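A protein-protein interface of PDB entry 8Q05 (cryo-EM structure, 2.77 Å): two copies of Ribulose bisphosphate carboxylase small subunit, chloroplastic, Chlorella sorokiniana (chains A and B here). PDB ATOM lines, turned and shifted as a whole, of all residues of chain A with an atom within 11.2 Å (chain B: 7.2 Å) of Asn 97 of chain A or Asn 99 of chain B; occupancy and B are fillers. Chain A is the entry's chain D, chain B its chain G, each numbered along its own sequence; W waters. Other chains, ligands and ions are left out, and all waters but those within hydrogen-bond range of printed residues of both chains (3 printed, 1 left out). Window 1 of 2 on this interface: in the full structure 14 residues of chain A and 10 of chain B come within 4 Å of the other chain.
The guanidinium group (NH2) of Arg 102 of chain B sits at hydrogen-bond distance from the backbone carbonyl oxygen (O) of Thr 107 of chain A, at 3.0 Å. The backbone carbonyl oxygen (O) of Tyr 110 of chain A sits at hydrogen-bond distance from the guanidinium group (NH1) of Arg 102 of chain B. The side-chain amide oxygen (OD1) of Asn 97 of chain A is in hydrogen-bond range of the guanidinium group (NH1) of Arg 102 of chain B (3.4 Å). The guanidinium group (NH1) of Arg 102 of chain B lies within hydrogen-bond range of the side-chain sulfur (SG) of Cys 100 of chain A.
The guanidinium group of Arg 114 of chain A lies within hydrogen-bond range of the backbone carbonyl oxygen of Tyr 111 of chain A. The side-chain carboxylate (OD2) of Asp 112 of chain B sits at hydrogen-bond distance from the side-chain amide nitrogen (ND2) of Asn 99 of chain B, at 2.8 Å. The side-chain carboxylate of Asp 112 of chain A is in hydrogen-bond range of the side-chain hydroxyl of Tyr 110 of chain A (3.3 Å).
Among the printed residues, pairs that only touch across the chains: Asn 97 of chain A with Asn 99 of chain B (3.5 Å), Val 101 of chain A with Val 101 of chain B (3.6 Å), Tyr 111 of chain A with Arg 102 of chain B (3.7 Å) and Cys 100 of chain A with Val 101 of chain B (3.8 Å).
Of chain B, only Asn 99 (3.5 Å) and Arg 102 (3.4 Å) come within 4 Å of Asn 97 of chain A. Of the printed residues of chain B, Cys 100 of chain A touches Val 101 and Arg 102. Of the printed residues of chain B, Val 101 of chain A touches Val 101 (3.6 Å). Of the printed residues of chain B, Thr 107 of chain A touches Arg 102. Of the printed residues of chain B, Tyr 111 of chain A touches Arg 102 (3.7 Å). Asn 99 of chain B touches one residue of chain A. No residue of chain A comes within 4 Å of Cys 100 of chain B. Val 101 of chain B touches just these residues of chain A: Cys 100 (3.8 Å) and Val 101 (3.6 Å). Of the printed residues of chain A, Arg 102 of chain B touches Asn 97, Cys 100, Thr 107, Tyr 110 and Tyr 111. No residue of chain A comes within 4 Å of Met 103 of chain B. The nearest printed residue of chain B that does not touch Val 101 of chain A is Arg 102 of chain B (6.6 Å).
Of the 22 printed residues of chain A, 6 touch a printed residue of chain B. Printed residues of chain A that touch a printed residue of chain B: Asn 97, Cys 100, Val 101, Thr 107, Tyr 110 and Tyr 111. Hydrophobic or aromatic side chains of chain A that line the printed part of chain B: Val 101 and Tyr 111. Hydrophobic or aromatic side chains of chain B that line the printed part of chain A: Val 101. Along chain B the printed residues that touch a printed residue of chain A span positions 99 to 102.
Cys 100 of chain A touches Val 101 of chain B, but with the chains exchanged Val 101 of chain A does not touch Cys 100 of chain B (8.0 Å). Cys 100 of chain A touches Arg 102 of chain B, but with the chains exchanged Arg 102 of chain A does not touch Cys 100 of chain B (10.0 Å). Val 101 of chain B touches its own counterpart, Val 101 of chain A. Thr 107 of chain A touches Arg 102 of chain B, but with the chains exchanged Arg 102 of chain A does not touch Thr 107 of chain B (13.8 Å). 12 positions are printed for both chains. Of the 8 pairs that touch across the chains among the printed residues, 1 has its exchanged pair printed and touching as well.
Water W1 bridges the backbone carbonyl oxygen of Glu 98 of chain B (2.8 Å) and the side-chain amide nitrogen of Asn 97 of chain A (3.4 Å). Water W3 lies within hydrogen-bond range of OG1 of Thr 106 of chain A, N of Thr 107 of chain A and O of Arg 102 of chain B. Water W2 lies within hydrogen-bond range of OD1 of Asn 99 of chain B (3.1 Å) and ND2 of Asn 97 of chain A (3.5 Å).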
ATOM      1  N   GLU A  91     -35.527 -15.141  14.220  1.00  0.00           N
ATOM      2  CA  GLU A  91     -34.245 -14.471  14.050  1.00  0.00           C
ATOM      3  C   GLU A  91     -33.169 -14.994  14.993  1.00  0.00           C
ATOM      4  O   GLU A  91     -31.981 -14.842  14.695  1.00  0.00           O
ATOM      5  CB  GLU A  91     -34.414 -12.962  14.238  1.00  0.00           C
ATOM      6  CG  GLU A  91     -34.615 -12.526  15.682  1.00  0.00           C
ATOM      7  CD  GLU A  91     -36.065 -12.615  16.120  1.00  0.00           C
ATOM      8  OE1 GLU A  91     -36.957 -12.428  15.268  1.00  0.00           O
ATOM      9  OE2 GLU A  91     -36.311 -12.874  17.318  1.00  0.00           O
ATOM     10  N   SER A  92     -33.545 -15.618  16.109  1.00  0.00           N
ATOM     11  CA  SER A  92     -32.570 -16.126  17.066  1.00  0.00           C
ATOM     12  C   SER A  92     -32.856 -17.574  17.440  1.00  0.00           C
ATOM     13  O   SER A  92     -32.615 -17.986  18.576  1.00  0.00           O
ATOM     14  CB  SER A  92     -32.529 -15.253  18.318  1.00  0.00           C
ATOM     15  OG  SER A  92     -33.803 -15.184  18.930  1.00  0.00           O
ATOM     16  N   ALA A  93     -33.365 -18.362  16.496  1.00  0.00           N
ATOM     17  CA  ALA A  93     -33.686 -19.760  16.746  1.00  0.00           C
ATOM     18  C   ALA A  93     -32.618 -20.719  16.245  1.00  0.00           C
ATOM     19  O   ALA A  93     -32.349 -21.730  16.896  1.00  0.00           O
ATOM     20  CB  ALA A  93     -35.026 -20.119  16.102  1.00  0.00           C
ATOM     21  N   TYR A  94     -32.003 -20.429  15.106  1.00  0.00           N
ATOM     22  CA  TYR A  94     -31.010 -21.305  14.506  1.00  0.00           C
ATOM     23  C   TYR A  94     -29.609 -20.872  14.913  1.00  0.00           C
ATOM     24  O   TYR A  94     -29.366 -19.705  15.222  1.00  0.00           O
ATOM     25  CB  TYR A  94     -31.134 -21.305  12.979  1.00  0.00           C
ATOM     26  CG  TYR A  94     -32.530 -21.001  12.491  1.00  0.00           C
ATOM     27  CD1 TYR A  94     -33.597 -21.823  12.828  1.00  0.00           C
ATOM     28  CD2 TYR A  94     -32.786 -19.879  11.719  1.00  0.00           C
ATOM     29  CE1 TYR A  94     -34.871 -21.546  12.397  1.00  0.00           C
ATOM     30  CE2 TYR A  94     -34.060 -19.591  11.285  1.00  0.00           C
ATOM     31  CZ  TYR A  94     -35.100 -20.428  11.628  1.00  0.00           C
ATOM     32  OH  TYR A  94     -36.373 -20.146  11.200  1.00  0.00           O
ATOM     33  N   THR A  95     -28.690 -21.834  14.918  1.00  0.00           N
ATOM     34  CA  THR A  95     -27.302 -21.546  15.247  1.00  0.00           C
ATOM     35  C   THR A  95     -26.684 -20.630  14.199  1.00  0.00           C
ATOM     36  O   THR A  95     -27.029 -20.678  13.017  1.00  0.00           O
ATOM     37  CB  THR A  95     -26.492 -22.838  15.352  1.00  0.00           C
ATOM     38  OG1 THR A  95     -26.460 -23.486  14.076  1.00  0.00           O
ATOM     39  CG2 THR A  95     -27.117 -23.781  16.369  1.00  0.00           C
ATOM     40  N   SER A  96     -25.757 -19.786  14.645  1.00  0.00           N
ATOM     41  CA  SER A  96     -25.143 -18.800  13.771  1.00  0.00           C
ATOM     42  C   SER A  96     -23.750 -18.470  14.282  1.00  0.00           C
ATOM     43  O   SER A  96     -23.388 -18.788  15.415  1.00  0.00           O
ATOM     44  CB  SER A  96     -26.001 -17.538  13.674  1.00  0.00           C
ATOM     45  OG  SER A  96     -26.174 -16.951  14.948  1.00  0.00           O
ATOM     46  N   ASN A  97     -22.964 -17.830  13.421  1.00  0.00           N
ATOM     47  CA  ASN A  97     -21.604 -17.409  13.729  1.00  0.00           C
ATOM     48  C   ASN A  97     -21.483 -15.891  13.719  1.00  0.00           C
ATOM     49  O   ASN A  97     -20.494 -15.336  13.242  1.00  0.00           O
ATOM     50  CB  ASN A  97     -20.603 -18.014  12.747  1.00  0.00           C
ATOM     51  CG  ASN A  97     -20.957 -19.425  12.339  1.00  0.00           C
ATOM     52  OD1 ASN A  97     -21.237 -20.275  13.179  1.00  0.00           O
ATOM     53  ND2 ASN A  97     -20.954 -19.679  11.040  1.00  0.00           N
ATOM     54  N   GLU A  98     -22.490 -15.193  14.246  1.00  0.00           N
ATOM     55  CA  GLU A  98     -22.508 -13.740  14.123  1.00  0.00           C
ATOM     56  C   GLU A  98     -21.434 -13.087  14.986  1.00  0.00           C
ATOM     57  O   GLU A  98     -20.839 -12.082  14.586  1.00  0.00           O
ATOM     58  CB  GLU A  98     -23.896 -13.200  14.464  1.00  0.00           C
ATOM     59  CG  GLU A  98     -24.315 -13.365  15.910  1.00  0.00           C
ATOM     60  CD  GLU A  98     -25.754 -12.961  16.144  1.00  0.00           C
ATOM     61  OE1 GLU A  98     -26.660 -13.709  15.718  1.00  0.00           O
ATOM     62  OE2 GLU A  98     -25.981 -11.893  16.750  1.00  0.00           O
ATOM     63  N   ASN A  99     -21.158 -13.648  16.160  1.00  0.00           N
ATOM     64  CA  ASN A  99     -20.212 -13.058  17.094  1.00  0.00           C
ATOM     65  C   ASN A  99     -18.799 -13.601  16.942  1.00  0.00           C
ATOM     66  O   ASN A  99     -17.896 -13.129  17.638  1.00  0.00           O
ATOM     67  CB  ASN A  99     -20.697 -13.265  18.528  1.00  0.00           C
ATOM     68  CG  ASN A  99     -21.854 -12.359  18.881  1.00  0.00           C
ATOM     69  OD1 ASN A  99     -21.717 -11.140  18.882  1.00  0.00           O
ATOM     70  ND2 ASN A  99     -23.005 -12.950  19.170  1.00  0.00           N
ATOM     71  N   CYS A 100     -18.581 -14.564  16.046  1.00  0.00           N
ATOM     72  CA  CYS A 100     -17.239 -15.081  15.812  1.00  0.00           C
ATOM     73  C   CYS A 100     -16.300 -14.019  15.262  1.00  0.00           C
ATOM     74  O   CYS A 100     -15.081 -14.195  15.328  1.00  0.00           O
ATOM     75  CB  CYS A 100     -17.290 -16.266  14.851  1.00  0.00           C
ATOM     76  SG  CYS A 100     -17.809 -17.811  15.604  1.00  0.00           S
ATOM     77  N   VAL A 101     -16.841 -12.922  14.729  1.00  0.00           N
ATOM     78  CA  VAL A 101     -16.022 -11.831  14.223  1.00  0.00           C
ATOM     79  C   VAL A 101     -15.236 -11.142  15.334  1.00  0.00           C
ATOM     80  O   VAL A 101     -14.227 -10.485  15.059  1.00  0.00           O
ATOM     81  CB  VAL A 101     -16.922 -10.839  13.462  1.00  0.00           C
ATOM     82  CG1 VAL A 101     -17.851 -10.102  14.421  1.00  0.00           C
ATOM     83  CG2 VAL A 101     -16.092  -9.868  12.652  1.00  0.00           C
ATOM     84  N   ARG A 102     -15.660 -11.284  16.585  1.00  0.00           N
ATOM     85  CA  ARG A 102     -15.002 -10.648  17.716  1.00  0.00           C
ATOM     86  C   ARG A 102     -13.923 -11.512  18.349  1.00  0.00           C
ATOM     87  O   ARG A 102     -13.317 -11.089  19.336  1.00  0.00           O
ATOM     88  CB  ARG A 102     -16.031 -10.281  18.786  1.00  0.00           C
ATOM     89  CG  ARG A 102     -17.003  -9.198  18.377  1.00  0.00           C
ATOM     90  CD  ARG A 102     -17.902  -8.817  19.533  1.00  0.00           C
ATOM     91  NE  ARG A 102     -17.137  -8.308  20.662  1.00  0.00           N
ATOM     92  CZ  ARG A 102     -16.621  -7.090  20.729  1.00  0.00           C
ATOM     93  NH1 ARG A 102     -16.794  -6.214  19.756  1.00  0.00           N
ATOM     94  NH2 ARG A 102     -15.907  -6.747  21.793  1.00  0.00           N
ATOM     95  N   MET A 103     -13.668 -12.702  17.821  1.00  0.00           N
ATOM     96  CA  MET A 103     -12.816 -13.671  18.488  1.00  0.00           C
ATOM     97  C   MET A 103     -11.558 -13.962  17.689  1.00  0.00           C
ATOM     98  O   MET A 103     -11.538 -13.863  16.461  1.00  0.00           O
ATOM     99  CB  MET A 103     -13.567 -14.963  18.745  1.00  0.00           C
ATOM    100  CG  MET A 103     -14.790 -14.739  19.572  1.00  0.00           C
ATOM    101  SD  MET A 103     -15.451 -16.250  20.253  1.00  0.00           S
ATOM    102  CE  MET A 103     -17.167 -15.868  20.066  1.00  0.00           C
ATOM    103  N   THR A 106      -9.234 -19.166  18.287  1.00  0.00           N
ATOM    104  CA  THR A 106     -10.101 -20.227  17.795  1.00  0.00           C
ATOM    105  C   THR A 106     -11.549 -19.875  18.099  1.00  0.00           C
ATOM    106  O   THR A 106     -11.837 -19.041  18.959  1.00  0.00           O
ATOM    107  CB  THR A 106      -9.738 -21.581  18.414  1.00  0.00           C
ATOM    108  OG1 THR A 106     -10.293 -22.634  17.620  1.00  0.00           O
ATOM    109  CG2 THR A 106     -10.270 -21.688  19.826  1.00  0.00           C
ATOM    110  N   THR A 107     -12.458 -20.514  17.360  1.00  0.00           N
ATOM    111  CA  THR A 107     -13.889 -20.456  17.636  1.00  0.00           C
ATOM    112  C   THR A 107     -14.477 -21.849  17.822  1.00  0.00           C
ATOM    113  O   THR A 107     -15.689 -22.029  17.686  1.00  0.00           O
ATOM    114  CB  THR A 107     -14.645 -19.715  16.529  1.00  0.00           C
ATOM    115  OG1 THR A 107     -14.522 -20.430  15.295  1.00  0.00           O
ATOM    116  CG2 THR A 107     -14.110 -18.307  16.354  1.00  0.00           C
ATOM    117  N   CYS A 108     -13.637 -22.835  18.126  1.00  0.00           N
ATOM    118  CA  CYS A 108     -14.097 -24.209  18.270  1.00  0.00           C
ATOM    119  C   CYS A 108     -15.141 -24.320  19.371  1.00  0.00           C
ATOM    120  O   CYS A 108     -14.951 -23.811  20.478  1.00  0.00           O
ATOM    121  CB  CYS A 108     -12.919 -25.130  18.577  1.00  0.00           C
ATOM    122  SG  CYS A 108     -11.727 -25.306  17.250  1.00  0.00           S
ATOM    123  N   LEU A 109     -16.252 -25.002  19.063  1.00  0.00           N
ATOM    124  CA  LEU A 109     -17.333 -25.267  20.060  1.00  0.00           C
ATOM    125  C   LEU A 109     -18.074 -23.985  20.461  1.00  0.00           C
ATOM    126  O   LEU A 109     -18.820 -24.040  21.453  1.00  0.00           O
ATOM    127  CB  LEU A 109     -16.756 -26.030  21.261  1.00  0.00           C
ATOM    128  CG  LEU A 109     -16.331 -27.464  20.944  1.00  0.00           C
ATOM    129  CD1 LEU A 109     -16.081 -28.264  22.211  1.00  0.00           C
ATOM    130  CD2 LEU A 109     -17.374 -28.156  20.080  1.00  0.00           C
ATOM    131  N   TYR A 110     -17.886 -22.884  19.731  1.00  0.00           N
ATOM    132  CA  TYR A 110     -18.672 -21.688  19.981  1.00  0.00           C
ATOM    133  C   TYR A 110     -19.699 -21.529  18.873  1.00  0.00           C
ATOM    134  O   TYR A 110     -19.344 -21.495  17.692  1.00  0.00           O
ATOM    135  CB  TYR A 110     -17.810 -20.427  20.063  1.00  0.00           C
ATOM    136  CG  TYR A 110     -18.651 -19.208  20.367  1.00  0.00           C
ATOM    137  CD1 TYR A 110     -18.878 -18.809  21.673  1.00  0.00           C
ATOM    138  CD2 TYR A 110     -19.258 -18.485  19.348  1.00  0.00           C
ATOM    139  CE1 TYR A 110     -19.663 -17.713  21.954  1.00  0.00           C
ATOM    140  CE2 TYR A 110     -20.052 -17.396  19.622  1.00  0.00           C
ATOM    141  CZ  TYR A 110     -20.245 -17.010  20.923  1.00  0.00           C
ATOM    142  OH  TYR A 110     -21.028 -15.918  21.192  1.00  0.00           O
ATOM    143  N   TYR A 111     -20.962 -21.411  19.260  1.00  0.00           N
ATOM    144  CA  TYR A 111     -22.042 -21.151  18.325  1.00  0.00           C
ATOM    145  C   TYR A 111     -23.045 -20.227  18.994  1.00  0.00           C
ATOM    146  O   TYR A 111     -23.293 -20.328  20.195  1.00  0.00           O
ATOM    147  CB  TYR A 111     -22.730 -22.445  17.874  1.00  0.00           C
ATOM    148  CG  TYR A 111     -21.789 -23.472  17.300  1.00  0.00           C
ATOM    149  CD1 TYR A 111     -21.430 -23.443  15.962  1.00  0.00           C
ATOM    150  CD2 TYR A 111     -21.252 -24.470  18.099  1.00  0.00           C
ATOM    151  CE1 TYR A 111     -20.567 -24.375  15.436  1.00  0.00           C
ATOM    152  CE2 TYR A 111     -20.387 -25.406  17.582  1.00  0.00           C
ATOM    153  CZ  TYR A 111     -20.050 -25.353  16.251  1.00  0.00           C
ATOM    154  OH  TYR A 111     -19.191 -26.290  15.732  1.00  0.00           O
ATOM    155  N   ASP A 112     -23.608 -19.321  18.211  1.00  0.00           N
ATOM    156  CA  ASP A 112     -24.613 -18.402  18.715  1.00  0.00           C
ATOM    157  C   ASP A 112     -25.986 -19.056  18.696  1.00  0.00           C
ATOM    158  O   ASP A 112     -26.215 -20.054  18.010  1.00  0.00           O
ATOM    159  CB  ASP A 112     -24.631 -17.118  17.889  1.00  0.00           C
ATOM    160  CG  ASP A 112     -23.677 -16.078  18.418  1.00  0.00           C
ATOM    161  OD1 ASP A 112     -22.730 -15.718  17.691  1.00  0.00           O
ATOM    162  OD2 ASP A 112     -23.870 -15.620  19.559  1.00  0.00           O
ATOM    163  N   ASN A 113     -26.900 -18.480  19.470  1.00  0.00           N
ATOM    164  CA  ASN A 113     -28.286 -18.920  19.593  1.00  0.00           C
ATOM    165  C   ASN A 113     -28.423 -20.306  20.205  1.00  0.00           C
ATOM    166  O   ASN A 113     -29.489 -20.915  20.103  1.00  0.00           O
ATOM    167  CB  ASN A 113     -29.017 -18.879  18.245  1.00  0.00           C
ATOM    168  CG  ASN A 113     -29.021 -17.505  17.632  1.00  0.00           C
ATOM    169  OD1 ASN A 113     -28.744 -16.518  18.305  1.00  0.00           O
ATOM    170  ND2 ASN A 113     -29.346 -17.428  16.351  1.00  0.00           N
ATOM    171  N   ARG A 114     -27.372 -20.835  20.829  1.00  0.00           N
ATOM    172  CA  ARG A 114     -27.541 -22.054  21.611  1.00  0.00           C
ATOM    173  C   ARG A 114     -28.450 -21.798  22.803  1.00  0.00           C
ATOM    174  O   ARG A 114     -29.280 -22.642  23.154  1.00  0.00           O
ATOM    175  CB  ARG A 114     -26.183 -22.588  22.062  1.00  0.00           C
ATOM    176  CG  ARG A 114     -25.512 -23.491  21.048  1.00  0.00           C
ATOM    177  CD  ARG A 114     -24.224 -24.071  21.586  1.00  0.00           C
ATOM    178  NE  ARG A 114     -23.288 -23.031  21.983  1.00  0.00           N
ATOM    179  CZ  ARG A 114     -21.979 -23.203  22.087  1.00  0.00           C
ATOM    180  NH1 ARG A 114     -21.416 -24.372  21.841  1.00  0.00           N
ATOM    181  NH2 ARG A 114     -21.217 -22.174  22.440  1.00  0.00           N
ATOM    182  N   SER B  96     -18.895 -17.995  -1.898  1.00  0.00           N
ATOM    183  CA  SER B  96     -19.022 -16.990  -0.855  1.00  0.00           C
ATOM    184  C   SER B  96     -17.997 -17.261   0.235  1.00  0.00           C
ATOM    185  O   SER B  96     -17.403 -18.336   0.306  1.00  0.00           O
ATOM    186  CB  SER B  96     -20.438 -16.970  -0.278  1.00  0.00           C
ATOM    187  OG  SER B  96     -20.771 -18.226   0.278  1.00  0.00           O
ATOM    188  N   ASN B  97     -17.790 -16.257   1.083  1.00  0.00           N
ATOM    189  CA  ASN B  97     -16.863 -16.329   2.206  1.00  0.00           C
ATOM    190  C   ASN B  97     -17.601 -16.228   3.534  1.00  0.00           C
ATOM    191  O   ASN B  97     -17.138 -15.576   4.469  1.00  0.00           O
ATOM    192  CB  ASN B  97     -15.805 -15.230   2.117  1.00  0.00           C
ATOM    193  CG  ASN B  97     -15.364 -14.950   0.700  1.00  0.00           C
ATOM    194  OD1 ASN B  97     -15.038 -15.862  -0.054  1.00  0.00           O
ATOM    195  ND2 ASN B  97     -15.358 -13.680   0.327  1.00  0.00           N
ATOM    196  N   GLU B  98     -18.763 -16.873   3.639  1.00  0.00           N
ATOM    197  CA  GLU B  98     -19.592 -16.687   4.824  1.00  0.00           C
ATOM    198  C   GLU B  98     -18.972 -17.339   6.055  1.00  0.00           C
ATOM    199  O   GLU B  98     -19.075 -16.803   7.163  1.00  0.00           O
ATOM    200  CB  GLU B  98     -21.002 -17.216   4.569  1.00  0.00           C
ATOM    201  CG  GLU B  98     -21.106 -18.715   4.388  1.00  0.00           C
ATOM    202  CD  GLU B  98     -22.496 -19.153   3.979  1.00  0.00           C
ATOM    203  OE1 GLU B  98     -22.878 -18.910   2.814  1.00  0.00           O
ATOM    204  OE2 GLU B  98     -23.207 -19.736   4.822  1.00  0.00           O
ATOM    205  N   ASN B  99     -18.311 -18.480   5.883  1.00  0.00           N
ATOM    206  CA  ASN B  99     -17.754 -19.225   7.002  1.00  0.00           C
ATOM    207  C   ASN B  99     -16.301 -18.879   7.292  1.00  0.00           C
ATOM    208  O   ASN B  99     -15.740 -19.402   8.258  1.00  0.00           O
ATOM    209  CB  ASN B  99     -17.890 -20.725   6.748  1.00  0.00           C
ATOM    210  CG  ASN B  99     -19.310 -21.213   6.923  1.00  0.00           C
ATOM    211  OD1 ASN B  99     -19.868 -21.136   8.014  1.00  0.00           O
ATOM    212  ND2 ASN B  99     -19.907 -21.706   5.847  1.00  0.00           N
ATOM    213  N   CYS B 100     -15.685 -18.006   6.495  1.00  0.00           N
ATOM    214  CA  CYS B 100     -14.314 -17.589   6.757  1.00  0.00           C
ATOM    215  C   CYS B 100     -14.179 -16.850   8.079  1.00  0.00           C
ATOM    216  O   CYS B 100     -13.066 -16.731   8.597  1.00  0.00           O
ATOM    217  CB  CYS B 100     -13.804 -16.704   5.621  1.00  0.00           C
ATOM    218  SG  CYS B 100     -13.303 -17.601   4.149  1.00  0.00           S
ATOM    219  N   VAL B 101     -15.288 -16.356   8.634  1.00  0.00           N
ATOM    220  CA  VAL B 101     -15.264 -15.678   9.921  1.00  0.00           C
ATOM    221  C   VAL B 101     -14.876 -16.618  11.058  1.00  0.00           C
ATOM    222  O   VAL B 101     -14.431 -16.158  12.114  1.00  0.00           O
ATOM    223  CB  VAL B 101     -16.636 -15.022  10.167  1.00  0.00           C
ATOM    224  CG1 VAL B 101     -17.710 -16.079  10.401  1.00  0.00           C
ATOM    225  CG2 VAL B 101     -16.570 -14.047  11.322  1.00  0.00           C
ATOM    226  N   ARG B 102     -15.017 -17.926  10.868  1.00  0.00           N
ATOM    227  CA  ARG B 102     -14.704 -18.908  11.894  1.00  0.00           C
ATOM    228  C   ARG B 102     -13.268 -19.404  11.834  1.00  0.00           C
ATOM    229  O   ARG B 102     -12.895 -20.263  12.637  1.00  0.00           O
ATOM    230  CB  ARG B 102     -15.645 -20.108  11.779  1.00  0.00           C
ATOM    231  CG  ARG B 102     -17.089 -19.806  12.107  1.00  0.00           C
ATOM    232  CD  ARG B 102     -17.922 -21.070  12.085  1.00  0.00           C
ATOM    233  NE  ARG B 102     -17.449 -22.040  13.062  1.00  0.00           N
ATOM    234  CZ  ARG B 102     -17.687 -21.968  14.364  1.00  0.00           C
ATOM    235  NH1 ARG B 102     -18.416 -20.994  14.879  1.00  0.00           N
ATOM    236  NH2 ARG B 102     -17.172 -22.889  15.167  1.00  0.00           N
ATOM    237  N   MET B 103     -12.457 -18.899  10.915  1.00  0.00           N
ATOM    238  CA  MET B 103     -11.147 -19.468  10.650  1.00  0.00           C
ATOM    239  C   MET B 103     -10.029 -18.496  10.984  1.00  0.00           C
ATOM    240  O   MET B 103     -10.197 -17.278  10.924  1.00  0.00           O
ATOM    241  CB  MET B 103     -11.029 -19.901   9.201  1.00  0.00           C
ATOM    242  CG  MET B 103     -12.078 -20.898   8.832  1.00  0.00           C
ATOM    243  SD  MET B 103     -11.721 -21.744   7.303  1.00  0.00           S
ATOM    244  CE  MET B 103     -13.371 -21.811   6.673  1.00  0.00           C
ATOM    245  N   THR B 107      -7.198 -18.620   5.000  1.00  0.00           N
ATOM    246  CA  THR B 107      -8.386 -19.115   4.312  1.00  0.00           C
ATOM    247  C   THR B 107      -8.085 -19.456   2.858  1.00  0.00           C
ATOM    248  O   THR B 107      -9.004 -19.521   2.038  1.00  0.00           O
ATOM    249  CB  THR B 107      -9.537 -18.106   4.384  1.00  0.00           C
ATOM    250  OG1 THR B 107      -9.171 -16.904   3.699  1.00  0.00           O
ATOM    251  CG2 THR B 107      -9.889 -17.784   5.822  1.00  0.00           C
ATOM    252  N   TYR B 110     -10.136 -21.923   0.398  1.00  0.00           N
ATOM    253  CA  TYR B 110     -11.419 -22.236   1.003  1.00  0.00           C
ATOM    254  C   TYR B 110     -12.474 -21.297   0.443  1.00  0.00           C
ATOM    255  O   TYR B 110     -12.323 -20.075   0.515  1.00  0.00           O
ATOM    256  CB  TYR B 110     -11.392 -22.123   2.528  1.00  0.00           C
ATOM    257  CG  TYR B 110     -12.727 -22.498   3.129  1.00  0.00           C
ATOM    258  CD1 TYR B 110     -12.998 -23.803   3.502  1.00  0.00           C
ATOM    259  CD2 TYR B 110     -13.736 -21.554   3.276  1.00  0.00           C
ATOM    260  CE1 TYR B 110     -14.222 -24.152   4.028  1.00  0.00           C
ATOM    261  CE2 TYR B 110     -14.964 -21.897   3.790  1.00  0.00           C
ATOM    262  CZ  TYR B 110     -15.200 -23.193   4.170  1.00  0.00           C
ATOM    263  OH  TYR B 110     -16.422 -23.530   4.693  1.00  0.00           O
ATOM    264  N   ASP B 112     -16.996 -21.154   0.095  1.00  0.00           N
ATOM    265  CA  ASP B 112     -18.281 -21.765   0.382  1.00  0.00           C
ATOM    266  C   ASP B 112     -19.059 -21.993  -0.905  1.00  0.00           C
ATOM    267  O   ASP B 112     -18.771 -21.399  -1.946  1.00  0.00           O
ATOM    268  CB  ASP B 112     -19.091 -20.893   1.338  1.00  0.00           C
ATOM    269  CG  ASP B 112     -18.818 -21.216   2.785  1.00  0.00           C
ATOM    270  OD1 ASP B 112     -18.310 -20.334   3.504  1.00  0.00           O
ATOM    271  OD2 ASP B 112     -19.111 -22.351   3.206  1.00  0.00           O
ATOM    272  N   ASN B 113     -20.052 -22.872  -0.820  1.00  0.00           N
ATOM    273  CA  ASN B 113     -20.944 -23.232  -1.918  1.00  0.00           C
ATOM    274  C   ASN B 113     -20.230 -23.923  -3.070  1.00  0.00           C
ATOM    275  O   ASN B 113     -20.787 -24.018  -4.165  1.00  0.00           O
ATOM    276  CB  ASN B 113     -21.714 -22.015  -2.447  1.00  0.00           C
ATOM    277  CG  ASN B 113     -22.538 -21.347  -1.381  1.00  0.00           C
ATOM    278  OD1 ASN B 113     -22.783 -21.921  -0.325  1.00  0.00           O
ATOM    279  ND2 ASN B 113     -22.985 -20.131  -1.653  1.00  0.00           N
HETATM  280  O   HOH W   1     -21.281 -17.000   8.950  1.00  0.00           O
HETATM  281  O   HOH W   2     -21.892 -22.759   9.777  1.00  0.00           O
HETATM  282  O   HOH W   3     -10.980 -21.624  14.894  1.00  0.00           O
